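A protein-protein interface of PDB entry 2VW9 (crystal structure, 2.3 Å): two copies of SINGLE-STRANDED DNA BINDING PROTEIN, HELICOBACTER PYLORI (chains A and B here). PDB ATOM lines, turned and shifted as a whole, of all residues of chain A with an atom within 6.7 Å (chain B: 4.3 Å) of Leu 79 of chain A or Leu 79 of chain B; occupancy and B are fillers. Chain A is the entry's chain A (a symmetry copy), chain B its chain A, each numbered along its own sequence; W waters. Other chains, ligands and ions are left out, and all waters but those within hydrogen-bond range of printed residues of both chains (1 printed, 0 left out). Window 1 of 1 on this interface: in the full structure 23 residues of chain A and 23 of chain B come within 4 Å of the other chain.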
ATOM      1  N   ASN A   3      19.527  26.971 -19.291  1.00  0.00           N
ATOM      2  CA  ASN A   3      20.799  27.472 -19.809  1.00  0.00           C
ATOM      3  C   ASN A   3      21.895  26.497 -19.352  1.00  0.00           C
ATOM      4  O   ASN A   3      22.344  26.553 -18.217  1.00  0.00           O
ATOM      5  CB  ASN A   3      21.067  28.895 -19.249  1.00  0.00           C
ATOM      6  CG  ASN A   3      22.332  29.548 -19.837  1.00  0.00           C
ATOM      7  OD1 ASN A   3      23.223  28.859 -20.320  1.00  0.00           O
ATOM      8  ND2 ASN A   3      22.421  30.873 -19.761  1.00  0.00           N
ATOM      9  N   LYS A   4      22.347  25.631 -20.250  1.00  0.00           N
ATOM     10  CA  LYS A   4      23.334  24.631 -19.884  1.00  0.00           C
ATOM     11  C   LYS A   4      24.505  24.502 -20.829  1.00  0.00           C
ATOM     12  O   LYS A   4      24.351  24.455 -22.050  1.00  0.00           O
ATOM     13  CB  LYS A   4      22.634  23.282 -19.762  1.00  0.00           C
ATOM     14  CG  LYS A   4      23.514  22.060 -19.832  1.00  0.00           C
ATOM     15  CD  LYS A   4      24.237  21.826 -18.525  1.00  0.00           C
ATOM     16  CE  LYS A   4      23.267  21.699 -17.357  1.00  0.00           C
ATOM     17  NZ  LYS A   4      23.978  21.208 -16.139  1.00  0.00           N
ATOM     18  N   VAL A   5      25.685  24.435 -20.228  1.00  0.00           N
ATOM     19  CA  VAL A   5      26.939  24.256 -20.945  1.00  0.00           C
ATOM     20  C   VAL A   5      27.684  23.064 -20.358  1.00  0.00           C
ATOM     21  O   VAL A   5      27.737  22.893 -19.143  1.00  0.00           O
ATOM     22  CB  VAL A   5      27.870  25.488 -20.826  1.00  0.00           C
ATOM     23  CG1 VAL A   5      29.238  25.169 -21.431  1.00  0.00           C
ATOM     24  CG2 VAL A   5      27.252  26.665 -21.549  1.00  0.00           C
ATOM     25  N   MET A   7      31.350  21.293 -21.215  1.00  0.00           N
ATOM     26  CA  MET A   7      32.547  21.282 -22.038  1.00  0.00           C
ATOM     27  C   MET A   7      33.731  20.587 -21.412  1.00  0.00           C
ATOM     28  O   MET A   7      33.973  20.703 -20.211  1.00  0.00           O
ATOM     29  CB  MET A   7      32.989  22.697 -22.350  1.00  0.00           C
ATOM     30  CG  MET A   7      32.175  23.432 -23.394  1.00  0.00           C
ATOM     31  SD  MET A   7      32.918  25.061 -23.710  1.00  0.00           S
ATOM     32  CE  MET A   7      34.642  24.736 -23.173  1.00  0.00           C
ATOM     33  N   THR A  33      39.018  24.180 -25.896  1.00  0.00           N
ATOM     34  CA  THR A  33      38.346  22.956 -26.291  1.00  0.00           C
ATOM     35  C   THR A  33      38.502  22.881 -27.777  1.00  0.00           C
ATOM     36  O   THR A  33      38.158  23.834 -28.458  1.00  0.00           O
ATOM     37  CB  THR A  33      36.862  23.016 -25.957  1.00  0.00           C
ATOM     38  OG1 THR A  33      36.719  23.229 -24.557  1.00  0.00           O
ATOM     39  CG2 THR A  33      36.201  21.721 -26.279  1.00  0.00           C
ATOM     40  N   GLU A  47      38.839  23.374 -35.017  1.00  0.00           N
ATOM     41  CA  GLU A  47      38.408  24.651 -34.501  1.00  0.00           C
ATOM     42  C   GLU A  47      38.821  24.591 -33.029  1.00  0.00           C
ATOM     43  O   GLU A  47      38.683  23.558 -32.399  1.00  0.00           O
ATOM     44  CB  GLU A  47      36.895  24.800 -34.570  1.00  0.00           C
ATOM     45  CG  GLU A  47      36.262  24.615 -35.909  1.00  0.00           C
ATOM     46  CD  GLU A  47      34.761  24.719 -35.800  1.00  0.00           C
ATOM     47  OE1 GLU A  47      34.275  25.807 -35.434  1.00  0.00           O
ATOM     48  OE2 GLU A  47      34.067  23.717 -36.064  1.00  0.00           O
ATOM     49  N   CYS A  49      38.078  26.363 -29.408  1.00  0.00           N
ATOM     50  CA  CYS A  49      37.292  27.339 -28.705  1.00  0.00           C
ATOM     51  C   CYS A  49      38.012  27.752 -27.424  1.00  0.00           C
ATOM     52  O   CYS A  49      38.306  26.924 -26.577  1.00  0.00           O
ATOM     53  CB  CYS A  49      35.890  26.777 -28.401  1.00  0.00           C
ATOM     54  SG  CYS A  49      34.835  27.979 -27.578  1.00  0.00           S
ATOM     55  N   ILE A  51      37.767  30.075 -24.095  1.00  0.00           N
ATOM     56  CA  ILE A  51      36.695  30.671 -23.312  1.00  0.00           C
ATOM     57  C   ILE A  51      37.038  30.624 -21.817  1.00  0.00           C
ATOM     58  O   ILE A  51      37.753  29.715 -21.345  1.00  0.00           O
ATOM     59  CB  ILE A  51      35.358  29.932 -23.552  1.00  0.00           C
ATOM     60  CG1 ILE A  51      34.202  30.749 -22.977  1.00  0.00           C
ATOM     61  CG2 ILE A  51      35.402  28.553 -22.914  1.00  0.00           C
ATOM     62  CD1 ILE A  51      32.941  30.688 -23.811  1.00  0.00           C
ATOM     63  N   GLY A  77      28.141  24.136 -16.453  1.00  0.00           N
ATOM     64  CA  GLY A  77      27.598  25.368 -15.921  1.00  0.00           C
ATOM     65  C   GLY A  77      26.602  26.013 -16.851  1.00  0.00           C
ATOM     66  O   GLY A  77      25.808  25.351 -17.516  1.00  0.00           O
ATOM     67  N   ARG A  78      26.654  27.335 -16.895  1.00  0.00           N
ATOM     68  CA  ARG A  78      25.752  28.097 -17.743  1.00  0.00           C
ATOM     69  C   ARG A  78      26.499  29.149 -18.571  1.00  0.00           C
ATOM     70  O   ARG A  78      27.638  29.504 -18.269  1.00  0.00           O
ATOM     71  CB  ARG A  78      24.672  28.770 -16.881  1.00  0.00           C
ATOM     72  CG  ARG A  78      25.192  29.779 -15.840  1.00  0.00           C
ATOM     73  CD  ARG A  78      24.012  30.460 -15.131  1.00  0.00           C
ATOM     74  NE  ARG A  78      24.419  31.571 -14.278  1.00  0.00           N
ATOM     75  CZ  ARG A  78      24.937  31.437 -13.061  1.00  0.00           C
ATOM     76  NH1 ARG A  78      25.105  30.238 -12.547  1.00  0.00           N
ATOM     77  NH2 ARG A  78      25.294  32.505 -12.364  1.00  0.00           N
ATOM     78  N   LEU A  79      25.866  29.625 -19.634  1.00  0.00           N
ATOM     79  CA  LEU A  79      26.481  30.656 -20.440  1.00  0.00           C
ATOM     80  C   LEU A  79      26.146  32.007 -19.808  1.00  0.00           C
ATOM     81  O   LEU A  79      25.015  32.259 -19.400  1.00  0.00           O
ATOM     82  CB  LEU A  79      26.000  30.582 -21.893  1.00  0.00           C
ATOM     83  CG  LEU A  79      27.045  30.002 -22.850  1.00  0.00           C
ATOM     84  CD1 LEU A  79      26.452  29.847 -24.242  1.00  0.00           C
ATOM     85  CD2 LEU A  79      28.269  30.913 -22.891  1.00  0.00           C
ATOM     86  N   THR A  80      27.153  32.863 -19.732  1.00  0.00           N
ATOM     87  CA  THR A  80      27.010  34.166 -19.107  1.00  0.00           C
ATOM     88  C   THR A  80      27.364  35.364 -19.981  1.00  0.00           C
ATOM     89  O   THR A  80      28.349  35.356 -20.720  1.00  0.00           O
ATOM     90  CB  THR A  80      27.875  34.216 -17.837  1.00  0.00           C
ATOM     91  OG1 THR A  80      27.420  33.218 -16.916  1.00  0.00           O
ATOM     92  CG2 THR A  80      27.822  35.611 -17.196  1.00  0.00           C
ATOM     93  N   TYR A  81      26.549  36.407 -19.875  1.00  0.00           N
ATOM     94  CA  TYR A  81      26.779  37.641 -20.620  1.00  0.00           C
ATOM     95  C   TYR A  81      27.161  38.750 -19.639  1.00  0.00           C
ATOM     96  O   TYR A  81      26.327  39.215 -18.872  1.00  0.00           O
ATOM     97  CB  TYR A  81      25.521  38.061 -21.394  1.00  0.00           C
ATOM     98  CG  TYR A  81      25.722  39.317 -22.233  1.00  0.00           C
ATOM     99  CD1 TYR A  81      26.690  39.359 -23.235  1.00  0.00           C
ATOM    100  CD2 TYR A  81      24.957  40.466 -22.011  1.00  0.00           C
ATOM    101  CE1 TYR A  81      26.894  40.498 -23.998  1.00  0.00           C
ATOM    102  CE2 TYR A  81      25.154  41.625 -22.766  1.00  0.00           C
ATOM    103  CZ  TYR A  81      26.123  41.628 -23.757  1.00  0.00           C
ATOM    104  OH  TYR A  81      26.340  42.742 -24.522  1.00  0.00           O
ATOM    105  N   HIS A  95      31.235  37.203 -22.961  1.00  0.00           N
ATOM    106  CA  HIS A  95      30.565  35.921 -22.822  1.00  0.00           C
ATOM    107  C   HIS A  95      31.513  35.004 -22.079  1.00  0.00           C
ATOM    108  O   HIS A  95      32.640  34.782 -22.523  1.00  0.00           O
ATOM    109  CB  HIS A  95      30.267  35.282 -24.178  1.00  0.00           C
ATOM    110  CG  HIS A  95      29.193  35.976 -24.949  1.00  0.00           C
ATOM    111  ND1 HIS A  95      27.860  35.907 -24.600  1.00  0.00           N
ATOM    112  CD2 HIS A  95      29.258  36.782 -26.032  1.00  0.00           C
ATOM    113  CE1 HIS A  95      27.154  36.645 -25.439  1.00  0.00           C
ATOM    114  NE2 HIS A  95      27.976  37.187 -26.315  1.00  0.00           N
ATOM    115  N   THR A  96      31.064  34.490 -20.945  1.00  0.00           N
ATOM    116  CA  THR A  96      31.857  33.554 -20.181  1.00  0.00           C
ATOM    117  C   THR A  96      30.954  32.391 -19.750  1.00  0.00           C
ATOM    118  O   THR A  96      29.747  32.406 -19.981  1.00  0.00           O
ATOM    119  CB  THR A  96      32.431  34.233 -18.918  1.00  0.00           C
ATOM    120  OG1 THR A  96      31.348  34.732 -18.134  1.00  0.00           O
ATOM    121  CG2 THR A  96      33.367  35.400 -19.286  1.00  0.00           C
ATOM    122  N   ILE A  97      31.553  31.370 -19.155  1.00  0.00           N
ATOM    123  CA  ILE A  97      30.781  30.264 -18.615  1.00  0.00           C
ATOM    124  C   ILE A  97      30.882  30.397 -17.094  1.00  0.00           C
ATOM    125  O   ILE A  97      31.974  30.612 -16.555  1.00  0.00           O
ATOM    126  CB  ILE A  97      31.377  28.871 -18.979  1.00  0.00           C
ATOM    127  CG1 ILE A  97      31.283  28.603 -20.474  1.00  0.00           C
ATOM    128  CG2 ILE A  97      30.681  27.774 -18.163  1.00  0.00           C
ATOM    129  CD1 ILE A  97      32.205  27.458 -20.889  1.00  0.00           C
ATOM    130  N   THR A  98      29.751  30.313 -16.407  1.00  0.00           N
ATOM    131  CA  THR A  98      29.793  30.322 -14.955  1.00  0.00           C
ATOM    132  C   THR A  98      29.638  28.842 -14.605  1.00  0.00           C
ATOM    133  O   THR A  98      28.601  28.247 -14.844  1.00  0.00           O
ATOM    134  CB  THR A  98      28.655  31.172 -14.349  1.00  0.00           C
ATOM    135  OG1 THR A  98      28.797  32.526 -14.786  1.00  0.00           O
ATOM    136  CG2 THR A  98      28.703  31.153 -12.826  1.00  0.00           C
ATOM    137  N   ASN B   3      31.782  19.304 -26.424  1.00  0.00           N
ATOM    138  CA  ASN B   3      31.422  20.719 -26.401  1.00  0.00           C
ATOM    139  C   ASN B   3      29.905  20.810 -26.630  1.00  0.00           C
ATOM    140  O   ASN B   3      29.438  20.717 -27.755  1.00  0.00           O
ATOM    141  CB  ASN B   3      32.187  21.472 -27.523  1.00  0.00           C
ATOM    142  CG  ASN B   3      31.957  22.995 -27.497  1.00  0.00           C
ATOM    143  OD1 ASN B   3      30.963  23.466 -26.958  1.00  0.00           O
ATOM    144  ND2 ASN B   3      32.858  23.754 -28.111  1.00  0.00           N
ATOM    145  N   VAL B   5      26.090  22.818 -25.739  1.00  0.00           N
ATOM    146  CA  VAL B   5      25.279  23.929 -25.264  1.00  0.00           C
ATOM    147  C   VAL B   5      23.806  23.591 -25.456  1.00  0.00           C
ATOM    148  O   VAL B   5      23.416  23.050 -26.486  1.00  0.00           O
ATOM    149  CB  VAL B   5      25.557  25.241 -26.040  1.00  0.00           C
ATOM    150  CG1 VAL B   5      24.547  26.315 -25.630  1.00  0.00           C
ATOM    151  CG2 VAL B   5      26.962  25.720 -25.744  1.00  0.00           C
ATOM    152  N   MET B   7      20.282  25.660 -24.675  1.00  0.00           N
ATOM    153  CA  MET B   7      19.652  26.863 -24.161  1.00  0.00           C
ATOM    154  C   MET B   7      18.251  27.103 -24.669  1.00  0.00           C
ATOM    155  O   MET B   7      17.952  26.865 -25.838  1.00  0.00           O
ATOM    156  CB  MET B   7      20.465  28.088 -24.530  1.00  0.00           C
ATOM    157  CG  MET B   7      21.732  28.308 -23.733  1.00  0.00           C
ATOM    158  SD  MET B   7      22.508  29.872 -24.242  1.00  0.00           S
ATOM    159  CE  MET B   7      21.045  30.748 -24.920  1.00  0.00           C
ATOM    160  N   CYS B  49      21.191  36.657 -20.632  1.00  0.00           N
ATOM    161  CA  CYS B  49      22.286  36.332 -21.503  1.00  0.00           C
ATOM    162  C   CYS B  49      21.879  36.575 -22.953  1.00  0.00           C
ATOM    163  O   CYS B  49      20.917  36.000 -23.438  1.00  0.00           O
ATOM    164  CB  CYS B  49      22.728  34.872 -21.284  1.00  0.00           C
ATOM    165  SG  CYS B  49      24.142  34.424 -22.302  1.00  0.00           S
ATOM    166  N   ILE B  51      23.114  36.336 -26.821  1.00  0.00           N
ATOM    167  CA  ILE B  51      24.101  35.561 -27.557  1.00  0.00           C
ATOM    168  C   ILE B  51      23.559  35.190 -28.944  1.00  0.00           C
ATOM    169  O   ILE B  51      22.336  35.030 -29.141  1.00  0.00           O
ATOM    170  CB  ILE B  51      24.472  34.270 -26.793  1.00  0.00           C
ATOM    171  CG1 ILE B  51      25.716  33.636 -27.416  1.00  0.00           C
ATOM    172  CG2 ILE B  51      23.309  33.291 -26.822  1.00  0.00           C
ATOM    173  CD1 ILE B  51      26.651  33.009 -26.404  1.00  0.00           C
ATOM    174  N   ARG B  78      26.959  23.787 -30.072  1.00  0.00           N
ATOM    175  CA  ARG B  78      28.267  23.879 -29.445  1.00  0.00           C
ATOM    176  C   ARG B  78      28.713  25.335 -29.264  1.00  0.00           C
ATOM    177  O   ARG B  78      28.175  26.246 -29.893  1.00  0.00           O
ATOM    178  CB  ARG B  78      29.301  23.108 -30.282  1.00  0.00           C
ATOM    179  CG  ARG B  78      29.507  23.627 -31.717  1.00  0.00           C
ATOM    180  CD  ARG B  78      30.642  22.848 -32.401  1.00  0.00           C
ATOM    181  NE  ARG B  78      31.032  23.415 -33.687  1.00  0.00           N
ATOM    182  CZ  ARG B  78      30.365  23.236 -34.823  1.00  0.00           C
ATOM    183  NH1 ARG B  78      29.276  22.498 -34.838  1.00  0.00           N
ATOM    184  NH2 ARG B  78      30.786  23.805 -35.943  1.00  0.00           N
ATOM    185  N   LEU B  79      29.677  25.555 -28.381  1.00  0.00           N
ATOM    186  CA  LEU B  79      30.188  26.893 -28.187  1.00  0.00           C
ATOM    187  C   LEU B  79      31.279  27.133 -29.230  1.00  0.00           C
ATOM    188  O   LEU B  79      32.123  26.276 -29.481  1.00  0.00           O
ATOM    189  CB  LEU B  79      30.722  27.080 -26.764  1.00  0.00           C
ATOM    190  CG  LEU B  79      29.798  27.913 -25.872  1.00  0.00           C
ATOM    191  CD1 LEU B  79      30.334  27.949 -24.449  1.00  0.00           C
ATOM    192  CD2 LEU B  79      29.680  29.328 -26.431  1.00  0.00           C
ATOM    193  N   THR B  80      31.239  28.313 -29.831  1.00  0.00           N
ATOM    194  CA  THR B  80      32.172  28.670 -30.885  1.00  0.00           C
ATOM    195  C   THR B  80      32.989  29.936 -30.648  1.00  0.00           C
ATOM    196  O   THR B  80      32.483  30.950 -30.169  1.00  0.00           O
ATOM    197  CB  THR B  80      31.405  28.827 -32.209  1.00  0.00           C
ATOM    198  OG1 THR B  80      30.792  27.578 -32.550  1.00  0.00           O
ATOM    199  CG2 THR B  80      32.344  29.294 -33.332  1.00  0.00           C
ATOM    200  N   THR B  96      30.123  32.563 -30.137  1.00  0.00           N
ATOM    201  CA  THR B  96      28.772  32.330 -30.599  1.00  0.00           C
ATOM    202  C   THR B  96      28.423  30.856 -30.349  1.00  0.00           C
ATOM    203  O   THR B  96      29.263  30.070 -29.919  1.00  0.00           O
ATOM    204  CB  THR B  96      28.659  32.618 -32.112  1.00  0.00           C
ATOM    205  OG1 THR B  96      29.582  31.782 -32.808  1.00  0.00           O
ATOM    206  CG2 THR B  96      28.979  34.092 -32.425  1.00  0.00           C
ATOM    207  N   ILE B  97      27.170  30.500 -30.588  1.00  0.00           N
ATOM    208  CA  ILE B  97      26.756  29.111 -30.484  1.00  0.00           C
ATOM    209  C   ILE B  97      26.499  28.651 -31.920  1.00  0.00           C
ATOM    210  O   ILE B  97      25.845  29.357 -32.697  1.00  0.00           O
ATOM    211  CB  ILE B  97      25.413  28.933 -29.713  1.00  0.00           C
ATOM    212  CG1 ILE B  97      25.561  29.315 -28.248  1.00  0.00           C
ATOM    213  CG2 ILE B  97      24.903  27.495 -29.875  1.00  0.00           C
ATOM    214  CD1 ILE B  97      24.198  29.532 -27.594  1.00  0.00           C
HETATM  215  O   HOH W   1      32.432  25.846 -33.313  1.00  0.00           O
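The side-chain sulfur (SG) of Cys 49 of chain B lies within hydrogen-bond range of the backbone carbonyl oxygen (O) of Leu 79 of chain A, 3.7 Å away.
OE2 of Glu 47 of chain A lies within salt-bridge range of NH2 of Arg 78 of chain B, at 3.3 Å.
The backbone carbonyl oxygen (O) of Leu 79 of chain B lies within hydrogen-bond range of the side-chain sulfur (SG) of Cys 49 of chain A.
N of Leu 79 of chain B sits at hydrogen-bond distance from OD1 of Asn 3 of chain B (2.8 Å).
OD1 of Asn 3 of chain A is in hydrogen-bond range of N of Leu 79 of chain A (2.8 Å).
The backbone carbonyl oxygen of Thr 33 of chain A is in hydrogen-bond range of the backbone NH of Cys 49 of chain A (2.7 Å).
Asn 3 of chain A touches Met 7 of chain B.
O of Lys 4 of chain A touches CA of Val 5 of chain B (3.4 Å).
CG of Met 7 of chain A touches OD1 of Asn 3 of chain B, at 3.8 Å.
Met 7 of chain A touches Leu 79 of chain B.
CD1 of Leu 79 of chain B touches CD1 of Ile 51 of chain A, 3.8 Å away.
SD of Met 7 of chain B touches CD1 of Leu 79 of chain A (3.9 Å).
Ile 51 of chain B touches Leu 79 of chain A (CD1 to CD1, 3.8 Å).
Leu 79 of chain B touches Leu 79 of chain A (CD1 to CD2, 3.9 Å).
Tyr 81 of chain A touches Cys 49 of chain B (CB to CA, 3.7 Å).
Ile 51 of chain B touches His 95 of chain A.
Leu 79 of chain A touches just these residues of chain B: Met 7 (3.9 Å), Cys 49 (3.7 Å), Ile 51 (3.8 Å) and Leu 79 (3.9 Å).
Leu 79 of chain B touches just these residues of chain A: Met 7, Cys 49, Ile 51 and Leu 79.
Of the printed residues of chain A, Ile 51 of chain B touches Leu 79 (3.8 Å) and His 95 (3.6 Å).
Of the printed residues of chain B, Ile 51 of chain A touches Leu 79 (3.8 Å).
Of the printed residues of chain B, Lys 4 of chain A touches Val 5 (3.4 Å).
Printed residues of chain B within 4 Å of Glu 47 of chain A: Arg 78.
Thr 80 of chain A touches none of the printed residues of chain B.
Hydrophobic or aromatic side chains of chain A that line the printed part of chain B: Met 7, Ile 51, Leu 79, Tyr 81 and His 95.
Hydrophobic or aromatic side chains of chain B that line the printed part of chain A: Met 7, Ile 51 and Leu 79.
Among the printed residues, Asp or Glu carboxylates within 4 Å of a Lys or Arg side-chain nitrogen of the other chain: Glu 47 of chain A with Arg 78 of chain B (3.3 Å).
Asn 3 of chain A touches Met 7 of chain B, and with the chains exchanged Met 7 of chain A touches Asn 3 of chain B.
Met 7 of chain A touches Leu 79 of chain B, and with the chains exchanged Leu 79 of chain A touches Met 7 of chain B.
Ile 51 of chain A touches Leu 79 of chain B, and with the chains exchanged Leu 79 of chain A touches Ile 51 of chain B.
Leu 79 of chain A touches its own counterpart, Leu 79 of chain B.
Of the 13 pairs that touch across the chains among the printed residues, 9 have their exchanged pair printed and touching as well.
Water W1 lies within hydrogen-bond range of OG1 of Thr 80 of chain B, OE1 of Glu 47 of chain A and NE of Arg 78 of chain B.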
